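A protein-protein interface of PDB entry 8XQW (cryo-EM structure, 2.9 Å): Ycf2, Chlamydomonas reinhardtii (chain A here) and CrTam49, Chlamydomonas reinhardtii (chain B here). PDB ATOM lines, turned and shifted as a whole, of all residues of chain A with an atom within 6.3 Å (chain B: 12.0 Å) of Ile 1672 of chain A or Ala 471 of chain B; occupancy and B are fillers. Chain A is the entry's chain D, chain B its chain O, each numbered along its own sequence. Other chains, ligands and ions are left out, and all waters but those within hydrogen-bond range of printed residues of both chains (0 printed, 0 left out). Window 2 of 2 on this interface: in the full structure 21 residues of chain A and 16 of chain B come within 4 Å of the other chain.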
ATOM      1  N   ASP A1670      19.604  22.391  -7.725  1.00  0.00           N
ATOM      2  CA  ASP A1670      18.799  21.802  -8.782  1.00  0.00           C
ATOM      3  C   ASP A1670      18.996  20.294  -8.794  1.00  0.00           C
ATOM      4  O   ASP A1670      19.986  19.779  -8.273  1.00  0.00           O
ATOM      5  CB  ASP A1670      19.179  22.402 -10.133  1.00  0.00           C
ATOM      6  CG  ASP A1670      18.070  22.290 -11.148  1.00  0.00           C
ATOM      7  OD1 ASP A1670      17.196  21.415 -10.980  1.00  0.00           O
ATOM      8  OD2 ASP A1670      18.069  23.079 -12.116  1.00  0.00           O
ATOM      9  N   PHE A1671      18.045  19.576  -9.383  1.00  0.00           N
ATOM     10  CA  PHE A1671      18.077  18.126  -9.259  1.00  0.00           C
ATOM     11  C   PHE A1671      18.537  17.441 -10.536  1.00  0.00           C
ATOM     12  O   PHE A1671      19.016  16.306 -10.480  1.00  0.00           O
ATOM     13  CB  PHE A1671      16.704  17.610  -8.847  1.00  0.00           C
ATOM     14  CG  PHE A1671      16.755  16.375  -8.005  1.00  0.00           C
ATOM     15  CD1 PHE A1671      17.536  16.337  -6.865  1.00  0.00           C
ATOM     16  CD2 PHE A1671      16.002  15.269  -8.331  1.00  0.00           C
ATOM     17  CE1 PHE A1671      17.581  15.209  -6.080  1.00  0.00           C
ATOM     18  CE2 PHE A1671      16.043  14.134  -7.545  1.00  0.00           C
ATOM     19  CZ  PHE A1671      16.836  14.106  -6.419  1.00  0.00           C
ATOM     20  N   ILE A1672      18.398  18.091 -11.691  1.00  0.00           N
ATOM     21  CA  ILE A1672      18.893  17.482 -12.922  1.00  0.00           C
ATOM     22  C   ILE A1672      20.389  17.649 -13.094  1.00  0.00           C
ATOM     23  O   ILE A1672      20.986  16.957 -13.924  1.00  0.00           O
ATOM     24  CB  ILE A1672      18.222  18.058 -14.179  1.00  0.00           C
ATOM     25  CG1 ILE A1672      18.534  19.543 -14.296  1.00  0.00           C
ATOM     26  CG2 ILE A1672      16.732  17.805 -14.151  1.00  0.00           C
ATOM     27  CD1 ILE A1672      18.061  20.146 -15.580  1.00  0.00           C
ATOM     28  N   THR A1673      21.014  18.547 -12.343  1.00  0.00           N
ATOM     29  CA  THR A1673      22.459  18.696 -12.375  1.00  0.00           C
ATOM     30  C   THR A1673      23.165  17.822 -11.354  1.00  0.00           C
ATOM     31  O   THR A1673      24.357  17.548 -11.512  1.00  0.00           O
ATOM     32  CB  THR A1673      22.849  20.153 -12.144  1.00  0.00           C
ATOM     33  OG1 THR A1673      24.265  20.234 -11.961  1.00  0.00           O
ATOM     34  CG2 THR A1673      22.167  20.690 -10.915  1.00  0.00           C
ATOM     35  N   ILE A1674      22.473  17.394 -10.306  1.00  0.00           N
ATOM     36  CA  ILE A1674      23.025  16.459  -9.341  1.00  0.00           C
ATOM     37  C   ILE A1674      22.971  15.030  -9.856  1.00  0.00           C
ATOM     38  O   ILE A1674      23.885  14.245  -9.613  1.00  0.00           O
ATOM     39  CB  ILE A1674      22.283  16.596  -7.997  1.00  0.00           C
ATOM     40  CG1 ILE A1674      22.440  18.011  -7.458  1.00  0.00           C
ATOM     41  CG2 ILE A1674      22.802  15.604  -6.991  1.00  0.00           C
ATOM     42  CD1 ILE A1674      23.871  18.423  -7.275  1.00  0.00           C
ATOM     43  N   ILE A1675      21.921  14.689 -10.591  1.00  0.00           N
ATOM     44  CA  ILE A1675      21.715  13.327 -11.065  1.00  0.00           C
ATOM     45  C   ILE A1675      22.402  13.146 -12.411  1.00  0.00           C
ATOM     46  O   ILE A1675      22.248  13.995 -13.299  1.00  0.00           O
ATOM     47  CB  ILE A1675      20.220  13.007 -11.158  1.00  0.00           C
ATOM     48  CG1 ILE A1675      19.594  13.044  -9.771  1.00  0.00           C
ATOM     49  CG2 ILE A1675      20.013  11.662 -11.756  1.00  0.00           C
ATOM     50  CD1 ILE A1675      18.213  12.464  -9.721  1.00  0.00           C
ATOM     51  N   PRO A1676      23.159  12.071 -12.610  1.00  0.00           N
ATOM     52  CA  PRO A1676      23.835  11.875 -13.895  1.00  0.00           C
ATOM     53  C   PRO A1676      22.850  11.524 -14.998  1.00  0.00           C
ATOM     54  O   PRO A1676      21.663  11.311 -14.758  1.00  0.00           O
ATOM     55  CB  PRO A1676      24.788  10.708 -13.617  1.00  0.00           C
ATOM     56  CG  PRO A1676      24.793  10.533 -12.138  1.00  0.00           C
ATOM     57  CD  PRO A1676      23.485  11.007 -11.654  1.00  0.00           C
ATOM     58  N   THR A1759      10.653  16.860 -13.997  1.00  0.00           N
ATOM     59  CA  THR A1759      11.974  17.456 -13.894  1.00  0.00           C
ATOM     60  C   THR A1759      11.953  18.954 -14.115  1.00  0.00           C
ATOM     61  O   THR A1759      12.968  19.518 -14.522  1.00  0.00           O
ATOM     62  CB  THR A1759      12.941  16.806 -14.882  1.00  0.00           C
ATOM     63  OG1 THR A1759      12.532  17.102 -16.219  1.00  0.00           O
ATOM     64  CG2 THR A1759      12.957  15.315 -14.689  1.00  0.00           C
ATOM     65  N   GLN A1760      10.824  19.607 -13.881  1.00  0.00           N
ATOM     66  CA  GLN A1760      10.791  21.054 -13.905  1.00  0.00           C
ATOM     67  C   GLN A1760      11.240  21.593 -12.552  1.00  0.00           C
ATOM     68  O   GLN A1760      11.205  20.878 -11.549  1.00  0.00           O
ATOM     69  CB  GLN A1760       9.389  21.552 -14.226  1.00  0.00           C
ATOM     70  CG  GLN A1760       8.834  21.016 -15.512  1.00  0.00           C
ATOM     71  CD  GLN A1760       7.663  21.823 -16.005  1.00  0.00           C
ATOM     72  OE1 GLN A1760       6.615  21.876 -15.366  1.00  0.00           O
ATOM     73  NE2 GLN A1760       7.837  22.470 -17.145  1.00  0.00           N
ATOM     74  N   PRO A1761      11.686  22.846 -12.494  1.00  0.00           N
ATOM     75  CA  PRO A1761      12.104  23.412 -11.211  1.00  0.00           C
ATOM     76  C   PRO A1761      10.928  23.566 -10.262  1.00  0.00           C
ATOM     77  O   PRO A1761       9.859  24.050 -10.634  1.00  0.00           O
ATOM     78  CB  PRO A1761      12.685  24.771 -11.600  1.00  0.00           C
ATOM     79  CG  PRO A1761      12.051  25.086 -12.894  1.00  0.00           C
ATOM     80  CD  PRO A1761      11.909  23.789 -13.600  1.00  0.00           C
ATOM     81  N   LEU A1765      13.302  26.886  -6.713  1.00  0.00           N
ATOM     82  CA  LEU A1765      14.053  27.424  -7.837  1.00  0.00           C
ATOM     83  C   LEU A1765      13.270  28.506  -8.564  1.00  0.00           C
ATOM     84  O   LEU A1765      13.851  29.488  -9.034  1.00  0.00           O
ATOM     85  CB  LEU A1765      14.428  26.305  -8.800  1.00  0.00           C
ATOM     86  CG  LEU A1765      15.776  25.623  -8.604  1.00  0.00           C
ATOM     87  CD1 LEU A1765      16.881  26.605  -8.860  1.00  0.00           C
ATOM     88  CD2 LEU A1765      15.898  25.035  -7.214  1.00  0.00           C
ATOM     89  N   GLN A1769      14.492  32.313  -9.061  1.00  0.00           N
ATOM     90  CA  GLN A1769      14.542  33.012 -10.340  1.00  0.00           C
ATOM     91  C   GLN A1769      13.846  34.362 -10.254  1.00  0.00           C
ATOM     92  O   GLN A1769      14.395  35.378 -10.693  1.00  0.00           O
ATOM     93  CB  GLN A1769      13.910  32.158 -11.437  1.00  0.00           C
ATOM     94  CG  GLN A1769      14.852  31.142 -12.057  1.00  0.00           C
ATOM     95  CD  GLN A1769      14.120  30.070 -12.846  1.00  0.00           C
ATOM     96  OE1 GLN A1769      13.106  30.336 -13.491  1.00  0.00           O
ATOM     97  NE2 GLN A1769      14.631  28.845 -12.790  1.00  0.00           N
ATOM     98  N   GLU B 466       1.217  25.279 -17.851  1.00  0.00           N
ATOM     99  CA  GLU B 466       2.240  25.659 -18.809  1.00  0.00           C
ATOM    100  C   GLU B 466       3.625  25.284 -18.302  1.00  0.00           C
ATOM    101  O   GLU B 466       3.883  25.229 -17.101  1.00  0.00           O
ATOM    102  CB  GLU B 466       2.173  27.153 -19.096  1.00  0.00           C
ATOM    103  CG  GLU B 466       1.006  27.538 -19.975  1.00  0.00           C
ATOM    104  CD  GLU B 466       0.779  29.031 -20.028  1.00  0.00           C
ATOM    105  OE1 GLU B 466       1.279  29.745 -19.135  1.00  0.00           O
ATOM    106  OE2 GLU B 466       0.092  29.495 -20.962  1.00  0.00           O
ATOM    107  N   LYS B 467       4.525  25.031 -19.244  1.00  0.00           N
ATOM    108  CA  LYS B 467       5.875  24.615 -18.913  1.00  0.00           C
ATOM    109  C   LYS B 467       6.709  25.795 -18.435  1.00  0.00           C
ATOM    110  O   LYS B 467       6.535  26.930 -18.886  1.00  0.00           O
ATOM    111  CB  LYS B 467       6.548  23.979 -20.124  1.00  0.00           C
ATOM    112  CG  LYS B 467       5.874  22.722 -20.614  1.00  0.00           C
ATOM    113  CD  LYS B 467       6.681  22.068 -21.710  1.00  0.00           C
ATOM    114  CE  LYS B 467       5.824  21.119 -22.510  1.00  0.00           C
ATOM    115  NZ  LYS B 467       6.575  20.557 -23.659  1.00  0.00           N
ATOM    116  N   THR B 468       7.627  25.516 -17.516  1.00  0.00           N
ATOM    117  CA  THR B 468       8.595  26.496 -17.047  1.00  0.00           C
ATOM    118  C   THR B 468       9.969  26.162 -17.610  1.00  0.00           C
ATOM    119  O   THR B 468      10.297  24.997 -17.840  1.00  0.00           O
ATOM    120  CB  THR B 468       8.664  26.540 -15.518  1.00  0.00           C
ATOM    121  OG1 THR B 468       9.543  25.511 -15.050  1.00  0.00           O
ATOM    122  CG2 THR B 468       7.293  26.328 -14.915  1.00  0.00           C
ATOM    123  N   ARG B 469      10.772  27.193 -17.818  1.00  0.00           N
ATOM    124  CA  ARG B 469      12.062  27.068 -18.473  1.00  0.00           C
ATOM    125  C   ARG B 469      13.168  26.859 -17.442  1.00  0.00           C
ATOM    126  O   ARG B 469      12.915  26.718 -16.243  1.00  0.00           O
ATOM    127  CB  ARG B 469      12.329  28.311 -19.324  1.00  0.00           C
ATOM    128  CG  ARG B 469      11.174  28.712 -20.224  1.00  0.00           C
ATOM    129  CD  ARG B 469      11.308  28.111 -21.620  1.00  0.00           C
ATOM    130  NE  ARG B 469      11.183  26.656 -21.598  1.00  0.00           N
ATOM    131  CZ  ARG B 469      10.226  25.978 -22.217  1.00  0.00           C
ATOM    132  NH1 ARG B 469       9.299  26.623 -22.910  1.00  0.00           N
ATOM    133  NH2 ARG B 469      10.195  24.657 -22.139  1.00  0.00           N
ATOM    134  N   ARG B 470      14.406  26.822 -17.930  1.00  0.00           N
ATOM    135  CA  ARG B 470      15.653  26.975 -17.187  1.00  0.00           C
ATOM    136  C   ARG B 470      16.016  25.809 -16.273  1.00  0.00           C
ATOM    137  O   ARG B 470      17.035  25.907 -15.586  1.00  0.00           O
ATOM    138  CB  ARG B 470      15.663  28.255 -16.341  1.00  0.00           C
ATOM    139  CG  ARG B 470      15.250  29.498 -17.096  1.00  0.00           C
ATOM    140  CD  ARG B 470      15.594  30.726 -16.298  1.00  0.00           C
ATOM    141  NE  ARG B 470      16.986  30.682 -15.872  1.00  0.00           N
ATOM    142  CZ  ARG B 470      17.544  31.545 -15.031  1.00  0.00           C
ATOM    143  NH1 ARG B 470      18.821  31.413 -14.709  1.00  0.00           N
ATOM    144  NH2 ARG B 470      16.833  32.536 -14.513  1.00  0.00           N
ATOM    145  N   ALA B 471      15.242  24.731 -16.222  1.00  0.00           N
ATOM    146  CA  ALA B 471      15.629  23.568 -15.418  1.00  0.00           C
ATOM    147  C   ALA B 471      14.835  22.330 -15.792  1.00  0.00           C
ATOM    148  O   ALA B 471      14.980  21.298 -15.141  1.00  0.00           O
ATOM    149  CB  ALA B 471      15.458  23.858 -13.938  1.00  0.00           C
ATOM    150  OXT ALA B 471      14.037  22.333 -16.727  1.00  0.00           O
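Of the 6 printed residues of chain B, 5 touch a printed residue of chain A. Among the printed residues, no Asp or Glu carboxylate lies within 4 Å of a Lys or Arg side-chain nitrogen of the other chain.
N of Thr 468 of chain B sits close to NE2 of Gln 1760 of chain A (3.1 Å). The backbone carbonyl oxygen (O) of Thr 1759 of chain A lies close to the chain-end carboxylate (O) of Ala 471 of chain B.
Among the printed residues, pairs that only touch across the chains: Asp 1670 of chain A with Ala 471 of chain B (3.3 Å), Ile 1672 of chain A with Ala 471 of chain B (3.3 Å), Gln 1760 of chain A with Lys 467 of chain B (3.4 Å), Pro 1761 of chain A with Thr 468 of chain B (3.3 Å), Pro 1761 of chain A with Arg 469 of chain B (3.8 Å), Pro 1761 of chain A with Ala 471 of chain B (3.6 Å) and Gln 1769 of chain A with Arg 470 of chain B (3.4 Å).
Asp 1670 of chain A touches one residue of chain B. No residue of chain B comes within 4 Å of Phe 1671 of chain A. No residue of chain B comes within 4 Å of Thr 1673 of chain A. No residue of chain B comes within 4 Å of Ile 1674 of chain A. No residue of chain B comes within 4 Å of Ile 1675 of chain A. Thr 1759 of chain A touches just one residue of chain B: Ala 471 (2.8 Å). Of the printed residues of chain B, Gln 1769 of chain A touches Arg 470 (3.4 Å). Glu 466 of chain B touches none of the printed residues of chain A. Of the printed residues of chain A, Lys 467 of chain B touches Gln 1760 (3.4 Å). Of the printed residues of chain A, Thr 468 of chain B touches Gln 1760 (3.1 Å) and Pro 1761 (3.3 Å). Printed residues of chain A within 4 Å of Arg 469 of chain B: Pro 1761 (3.8 Å). Of the printed residues of chain A, Arg 470 of chain B touches Gln 1769. Ala 471 of chain B touches four residues of chain A. The nearest residue of chain B that does not touch Ile 1672 of chain A is Arg 470 of chain B (5.9 Å). The nearest residue of chain A that does not touch Ala 471 of chain B is Gln 1760 of chain A (4.4 Å). The nearest printed residue of chain A that does not touch Lys 467 of chain B is Pro 1761 of chain A (7.4 Å).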
